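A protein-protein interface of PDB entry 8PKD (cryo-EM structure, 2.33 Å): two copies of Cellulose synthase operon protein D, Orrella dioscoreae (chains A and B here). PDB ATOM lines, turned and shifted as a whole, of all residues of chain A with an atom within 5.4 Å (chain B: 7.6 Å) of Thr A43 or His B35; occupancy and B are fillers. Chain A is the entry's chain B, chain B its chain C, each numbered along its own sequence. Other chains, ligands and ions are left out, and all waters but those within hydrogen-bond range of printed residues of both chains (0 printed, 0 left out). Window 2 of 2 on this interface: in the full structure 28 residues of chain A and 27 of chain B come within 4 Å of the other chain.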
ATOM      1  N   PRO A  38     -15.524  30.216   2.270  1.00  0.00           N
ATOM      2  CA  PRO A  38     -15.710  29.386   3.473  1.00  0.00           C
ATOM      3  C   PRO A  38     -17.077  28.732   3.580  1.00  0.00           C
ATOM      4  O   PRO A  38     -17.166  27.602   4.073  1.00  0.00           O
ATOM      5  CB  PRO A  38     -15.470  30.380   4.613  1.00  0.00           C
ATOM      6  CG  PRO A  38     -14.547  31.376   4.036  1.00  0.00           C
ATOM      7  CD  PRO A  38     -14.963  31.535   2.604  1.00  0.00           C
ATOM      8  N   GLU A  39     -18.148  29.400   3.145  1.00  0.00           N
ATOM      9  CA  GLU A  39     -19.475  28.802   3.247  1.00  0.00           C
ATOM     10  C   GLU A  39     -19.607  27.588   2.335  1.00  0.00           C
ATOM     11  O   GLU A  39     -20.202  26.572   2.720  1.00  0.00           O
ATOM     12  CB  GLU A  39     -20.543  29.844   2.923  1.00  0.00           C
ATOM     13  CG  GLU A  39     -21.961  29.426   3.278  1.00  0.00           C
ATOM     14  CD  GLU A  39     -22.637  28.638   2.171  1.00  0.00           C
ATOM     15  OE1 GLU A  39     -22.292  28.853   0.990  1.00  0.00           O
ATOM     16  OE2 GLU A  39     -23.512  27.804   2.484  1.00  0.00           O
ATOM     17  N   GLN A  40     -19.064  27.679   1.122  1.00  0.00           N
ATOM     18  CA  GLN A  40     -19.093  26.539   0.213  1.00  0.00           C
ATOM     19  C   GLN A  40     -18.319  25.365   0.790  1.00  0.00           C
ATOM     20  O   GLN A  40     -18.755  24.211   0.694  1.00  0.00           O
ATOM     21  CB  GLN A  40     -18.526  26.946  -1.144  1.00  0.00           C
ATOM     22  CG  GLN A  40     -19.343  28.001  -1.857  1.00  0.00           C
ATOM     23  CD  GLN A  40     -18.713  28.443  -3.159  1.00  0.00           C
ATOM     24  OE1 GLN A  40     -17.619  28.009  -3.509  1.00  0.00           O
ATOM     25  NE2 GLN A  40     -19.402  29.312  -3.883  1.00  0.00           N
ATOM     26  N   LEU A  41     -17.167  25.642   1.401  1.00  0.00           N
ATOM     27  CA  LEU A  41     -16.397  24.581   2.038  1.00  0.00           C
ATOM     28  C   LEU A  41     -17.160  23.977   3.207  1.00  0.00           C
ATOM     29  O   LEU A  41     -17.094  22.765   3.438  1.00  0.00           O
ATOM     30  CB  LEU A  41     -15.044  25.120   2.490  1.00  0.00           C
ATOM     31  CG  LEU A  41     -14.060  25.423   1.362  1.00  0.00           C
ATOM     32  CD1 LEU A  41     -12.729  25.897   1.916  1.00  0.00           C
ATOM     33  CD2 LEU A  41     -13.869  24.197   0.489  1.00  0.00           C
ATOM     34  N   ARG A  42     -17.886  24.806   3.959  1.00  0.00           N
ATOM     35  CA  ARG A  42     -18.695  24.286   5.053  1.00  0.00           C
ATOM     36  C   ARG A  42     -19.770  23.342   4.535  1.00  0.00           C
ATOM     37  O   ARG A  42     -20.000  22.276   5.114  1.00  0.00           O
ATOM     38  CB  ARG A  42     -19.327  25.435   5.837  1.00  0.00           C
ATOM     39  CG  ARG A  42     -18.394  26.081   6.842  1.00  0.00           C
ATOM     40  CD  ARG A  42     -19.150  26.973   7.804  1.00  0.00           C
ATOM     41  NE  ARG A  42     -19.856  26.199   8.815  1.00  0.00           N
ATOM     42  CZ  ARG A  42     -19.303  25.744   9.932  1.00  0.00           C
ATOM     43  NH1 ARG A  42     -18.031  25.970  10.213  1.00  0.00           N
ATOM     44  NH2 ARG A  42     -20.043  25.045  10.786  1.00  0.00           N
ATOM     45  N   THR A  43     -20.435  23.715   3.442  1.00  0.00           N
ATOM     46  CA  THR A  43     -21.444  22.836   2.854  1.00  0.00           C
ATOM     47  C   THR A  43     -20.821  21.527   2.380  1.00  0.00           C
ATOM     48  O   THR A  43     -21.363  20.436   2.620  1.00  0.00           O
ATOM     49  CB  THR A  43     -22.147  23.547   1.700  1.00  0.00           C
ATOM     50  OG1 THR A  43     -23.027  24.549   2.221  1.00  0.00           O
ATOM     51  CG2 THR A  43     -22.950  22.562   0.876  1.00  0.00           C
ATOM     52  N   LEU A  44     -19.670  21.620   1.712  1.00  0.00           N
ATOM     53  CA  LEU A  44     -18.996  20.428   1.211  1.00  0.00           C
ATOM     54  C   LEU A  44     -18.622  19.485   2.346  1.00  0.00           C
ATOM     55  O   LEU A  44     -18.882  18.276   2.276  1.00  0.00           O
ATOM     56  CB  LEU A  44     -17.754  20.842   0.423  1.00  0.00           C
ATOM     57  CG  LEU A  44     -16.909  19.772  -0.261  1.00  0.00           C
ATOM     58  CD1 LEU A  44     -17.715  19.051  -1.322  1.00  0.00           C
ATOM     59  CD2 LEU A  44     -15.666  20.400  -0.859  1.00  0.00           C
ATOM     60  N   LEU A  45     -18.036  20.022   3.417  1.00  0.00           N
ATOM     61  CA  LEU A  45     -17.630  19.176   4.530  1.00  0.00           C
ATOM     62  C   LEU A  45     -18.826  18.667   5.325  1.00  0.00           C
ATOM     63  O   LEU A  45     -18.754  17.581   5.908  1.00  0.00           O
ATOM     64  CB  LEU A  45     -16.654  19.921   5.440  1.00  0.00           C
ATOM     65  CG  LEU A  45     -15.170  19.902   5.058  1.00  0.00           C
ATOM     66  CD1 LEU A  45     -14.634  18.485   5.121  1.00  0.00           C
ATOM     67  CD2 LEU A  45     -14.903  20.502   3.690  1.00  0.00           C
ATOM     68  N   ARG A  46     -19.933  19.412   5.357  1.00  0.00           N
ATOM     69  CA  ARG A  46     -21.138  18.891   5.995  1.00  0.00           C
ATOM     70  C   ARG A  46     -21.679  17.686   5.239  1.00  0.00           C
ATOM     71  O   ARG A  46     -22.073  16.683   5.853  1.00  0.00           O
ATOM     72  CB  ARG A  46     -22.198  19.987   6.098  1.00  0.00           C
ATOM     73  CG  ARG A  46     -23.376  19.617   6.982  1.00  0.00           C
ATOM     74  CD  ARG A  46     -24.110  20.841   7.497  1.00  0.00           C
ATOM     75  NE  ARG A  46     -23.965  21.989   6.612  1.00  0.00           N
ATOM     76  CZ  ARG A  46     -23.572  23.192   7.006  1.00  0.00           C
ATOM     77  NH1 ARG A  46     -23.273  23.443   8.270  1.00  0.00           N
ATOM     78  NH2 ARG A  46     -23.475  24.170   6.109  1.00  0.00           N
ATOM     79  N   GLU A  47     -21.703  17.758   3.908  1.00  0.00           N
ATOM     80  CA  GLU A  47     -22.132  16.596   3.135  1.00  0.00           C
ATOM     81  C   GLU A  47     -21.161  15.434   3.316  1.00  0.00           C
ATOM     82  O   GLU A  47     -21.576  14.267   3.389  1.00  0.00           O
ATOM     83  CB  GLU A  47     -22.273  16.959   1.660  1.00  0.00           C
ATOM     84  CG  GLU A  47     -23.124  15.977   0.879  1.00  0.00           C
ATOM     85  CD  GLU A  47     -22.820  15.991  -0.602  1.00  0.00           C
ATOM     86  OE1 GLU A  47     -22.977  17.059  -1.226  1.00  0.00           O
ATOM     87  OE2 GLU A  47     -22.425  14.937  -1.140  1.00  0.00           O
ATOM     88  N   ALA A  48     -19.863  15.734   3.395  1.00  0.00           N
ATOM     89  CA  ALA A  48     -18.883  14.687   3.661  1.00  0.00           C
ATOM     90  C   ALA A  48     -19.139  14.026   5.009  1.00  0.00           C
ATOM     91  O   ALA A  48     -19.037  12.802   5.142  1.00  0.00           O
ATOM     92  CB  ALA A  48     -17.469  15.262   3.605  1.00  0.00           C
ATOM     93  N   ALA B  29     -14.113  12.517  -0.541  1.00  0.00           N
ATOM     94  CA  ALA B  29     -14.097  12.235  -1.970  1.00  0.00           C
ATOM     95  C   ALA B  29     -15.507  12.025  -2.503  1.00  0.00           C
ATOM     96  O   ALA B  29     -15.828  12.458  -3.615  1.00  0.00           O
ATOM     97  CB  ALA B  29     -13.228  11.011  -2.255  1.00  0.00           C
ATOM     98  N   GLN B  30     -16.360  11.353  -1.729  1.00  0.00           N
ATOM     99  CA  GLN B  30     -17.745  11.168  -2.147  1.00  0.00           C
ATOM    100  C   GLN B  30     -18.456  12.504  -2.297  1.00  0.00           C
ATOM    101  O   GLN B  30     -19.164  12.735  -3.288  1.00  0.00           O
ATOM    102  CB  GLN B  30     -18.480  10.280  -1.145  1.00  0.00           C
ATOM    103  CG  GLN B  30     -19.909   9.960  -1.531  1.00  0.00           C
ATOM    104  CD  GLN B  30     -20.001   8.826  -2.525  1.00  0.00           C
ATOM    105  OE1 GLN B  30     -20.484   9.005  -3.642  1.00  0.00           O
ATOM    106  NE2 GLN B  30     -19.538   7.649  -2.125  1.00  0.00           N
ATOM    107  N   SER B  31     -18.275  13.400  -1.327  1.00  0.00           N
ATOM    108  CA  SER B  31     -18.904  14.715  -1.415  1.00  0.00           C
ATOM    109  C   SER B  31     -18.375  15.497  -2.610  1.00  0.00           C
ATOM    110  O   SER B  31     -19.145  16.145  -3.333  1.00  0.00           O
ATOM    111  CB  SER B  31     -18.682  15.490  -0.119  1.00  0.00           C
ATOM    112  OG  SER B  31     -19.452  16.678  -0.098  1.00  0.00           O
ATOM    113  N   LEU B  32     -17.060  15.440  -2.840  1.00  0.00           N
ATOM    114  CA  LEU B  32     -16.474  16.131  -3.981  1.00  0.00           C
ATOM    115  C   LEU B  32     -17.033  15.603  -5.295  1.00  0.00           C
ATOM    116  O   LEU B  32     -17.345  16.381  -6.203  1.00  0.00           O
ATOM    117  CB  LEU B  32     -14.954  15.988  -3.952  1.00  0.00           C
ATOM    118  CG  LEU B  32     -14.185  16.899  -2.999  1.00  0.00           C
ATOM    119  CD1 LEU B  32     -12.752  16.432  -2.868  1.00  0.00           C
ATOM    120  CD2 LEU B  32     -14.232  18.330  -3.487  1.00  0.00           C
ATOM    121  N   THR B  33     -17.165  14.281  -5.417  1.00  0.00           N
ATOM    122  CA  THR B  33     -17.726  13.704  -6.632  1.00  0.00           C
ATOM    123  C   THR B  33     -19.183  14.100  -6.819  1.00  0.00           C
ATOM    124  O   THR B  33     -19.612  14.355  -7.950  1.00  0.00           O
ATOM    125  CB  THR B  33     -17.592  12.184  -6.613  1.00  0.00           C
ATOM    126  OG1 THR B  33     -18.070  11.676  -5.362  1.00  0.00           O
ATOM    127  CG2 THR B  33     -16.145  11.777  -6.801  1.00  0.00           C
ATOM    128  N   ASN B  34     -19.957  14.147  -5.734  1.00  0.00           N
ATOM    129  CA  ASN B  34     -21.344  14.581  -5.848  1.00  0.00           C
ATOM    130  C   ASN B  34     -21.436  16.028  -6.314  1.00  0.00           C
ATOM    131  O   ASN B  34     -22.314  16.373  -7.112  1.00  0.00           O
ATOM    132  CB  ASN B  34     -22.073  14.406  -4.518  1.00  0.00           C
ATOM    133  CG  ASN B  34     -22.380  12.957  -4.208  1.00  0.00           C
ATOM    134  OD1 ASN B  34     -21.923  12.414  -3.204  1.00  0.00           O
ATOM    135  ND2 ASN B  34     -23.160  12.321  -5.071  1.00  0.00           N
ATOM    136  N   HIS B  35     -20.542  16.890  -5.830  1.00  0.00           N
ATOM    137  CA  HIS B  35     -20.669  18.310  -6.140  1.00  0.00           C
ATOM    138  C   HIS B  35     -20.021  18.683  -7.469  1.00  0.00           C
ATOM    139  O   HIS B  35     -20.583  19.482  -8.226  1.00  0.00           O
ATOM    140  CB  HIS B  35     -20.072  19.145  -5.011  1.00  0.00           C
ATOM    141  CG  HIS B  35     -21.021  19.393  -3.883  1.00  0.00           C
ATOM    142  ND1 HIS B  35     -20.862  20.427  -2.988  1.00  0.00           N
ATOM    143  CD2 HIS B  35     -22.150  18.745  -3.513  1.00  0.00           C
ATOM    144  CE1 HIS B  35     -21.848  20.401  -2.109  1.00  0.00           C
ATOM    145  NE2 HIS B  35     -22.643  19.390  -2.405  1.00  0.00           N
ATOM    146  N   PHE B  36     -18.851  18.131  -7.777  1.00  0.00           N
ATOM    147  CA  PHE B  36     -18.063  18.593  -8.909  1.00  0.00           C
ATOM    148  C   PHE B  36     -17.840  17.473  -9.915  1.00  0.00           C
ATOM    149  O   PHE B  36     -17.897  16.286  -9.589  1.00  0.00           O
ATOM    150  CB  PHE B  36     -16.712  19.149  -8.454  1.00  0.00           C
ATOM    151  CG  PHE B  36     -16.812  20.135  -7.336  1.00  0.00           C
ATOM    152  CD1 PHE B  36     -17.326  21.395  -7.555  1.00  0.00           C
ATOM    153  CD2 PHE B  36     -16.388  19.801  -6.066  1.00  0.00           C
ATOM    154  CE1 PHE B  36     -17.419  22.305  -6.528  1.00  0.00           C
ATOM    155  CE2 PHE B  36     -16.479  20.707  -5.035  1.00  0.00           C
ATOM    156  CZ  PHE B  36     -16.996  21.960  -5.265  1.00  0.00           C
ATOM    157  N   SER B  37     -17.587  17.881 -11.155  1.00  0.00           N
ATOM    158  CA  SER B  37     -17.268  16.980 -12.248  1.00  0.00           C
ATOM    159  C   SER B  37     -15.813  16.532 -12.164  1.00  0.00           C
ATOM    160  O   SER B  37     -15.001  17.158 -11.479  1.00  0.00           O
ATOM    161  CB  SER B  37     -17.530  17.670 -13.582  1.00  0.00           C
ATOM    162  OG  SER B  37     -16.723  18.825 -13.722  1.00  0.00           O
ATOM    163  N   GLN B  40     -13.096  19.318 -13.017  1.00  0.00           N
ATOM    164  CA  GLN B  40     -12.891  20.310 -11.970  1.00  0.00           C
ATOM    165  C   GLN B  40     -12.109  19.721 -10.807  1.00  0.00           C
ATOM    166  O   GLN B  40     -11.248  20.391 -10.222  1.00  0.00           O
ATOM    167  CB  GLN B  40     -14.235  20.858 -11.498  1.00  0.00           C
ATOM    168  CG  GLN B  40     -15.094  21.409 -12.615  1.00  0.00           C
ATOM    169  CD  GLN B  40     -16.481  21.786 -12.151  1.00  0.00           C
ATOM    170  OE1 GLN B  40     -17.411  20.986 -12.228  1.00  0.00           O
ATOM    171  NE2 GLN B  40     -16.629  23.010 -11.665  1.00  0.00           N
ATOM    172  N   LEU B  41     -12.393  18.466 -10.456  1.00  0.00           N
ATOM    173  CA  LEU B  41     -11.626  17.805  -9.409  1.00  0.00           C
ATOM    174  C   LEU B  41     -10.170  17.635  -9.822  1.00  0.00           C
ATOM    175  O   LEU B  41      -9.265  17.769  -8.992  1.00  0.00           O
ATOM    176  CB  LEU B  41     -12.254  16.455  -9.072  1.00  0.00           C
ATOM    177  CG  LEU B  41     -13.565  16.513  -8.292  1.00  0.00           C
ATOM    178  CD1 LEU B  41     -14.051  15.116  -7.955  1.00  0.00           C
ATOM    179  CD2 LEU B  41     -13.392  17.337  -7.030  1.00  0.00           C
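CE1 of His B35 touches CG2 of Thr A43, 3.8 Å away.
CD2 of Leu B32 touches CD2 of Leu A44, at 3.6 Å.
ND1 of His B35 touches CD1 of Leu A44 (3.8 Å).
Glu A47 touches Ser B31 (CB to OG, 3.3 Å).
Ser B31 touches Ala A48.
Along chain B the printed residues that touch a printed residue of chain A span positions 31 to 35.
Of the 11 printed residues of chain A, 4 touch a printed residue of chain B.
Hydrophobic or aromatic side chains of chain A that line the printed part of chain B: Leu A44 and Ala A48.
Among the printed residues, 8 pairs touch across the chains.
The side-chain carboxylate (OE2) of Glu A39 lies within hydrogen-bond range of the side-chain hydroxyl (OG1) of Thr A43, at 3.3 Å.
The backbone carbonyl oxygen of Gln B30 lies close to the side-chain amide oxygen of Asn B34, 2.8 Å away.
The backbone carbonyl oxygen of Leu A44 sits at hydrogen-bond distance from the side-chain hydroxyl of Ser B31, 2.9 Å away.
The side-chain amide oxygen (OD1) of Asn B34 lies close to the side-chain carboxylate (OE2) of Glu A47, at 3.3 Å.
The side-chain carboxylate of Glu A47 lies within hydrogen-bond range of a ring nitrogen (NE2) of His B35, at 2.6 Å.
Positions printed for both chains: 40 and 41.
Of the 8 pairs that touch across the chains among the printed residues, none has its exchanged pair printed and touching as well.
Of chain B, only His B35 (3.8 Å) comes within 4 Å of Thr A43.
Printed residues of chain A within 4 Å of His B35: Thr A43, Leu A44 and Glu A47.
Of the printed residues of chain A, Leu B32 touches Leu A44.
Printed residues of chain B within 4 Å of Glu A47: Ser B31, Asn B34 and His B35.
Printed residues of chain A within 4 Å of Asn B34: Glu A47 (3.3 Å).
Printed residues of chain A within 4 Å of Ser B31: Leu A44 (2.9 Å), Glu A47 (3.3 Å) and Ala A48 (3.6 Å).
The nearest residue of chain B that does not touch Thr A43 is Ser B31 (5.0 Å).
The nearest printed residue of chain A that does not touch His B35 is Gln A40 (5.7 Å).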
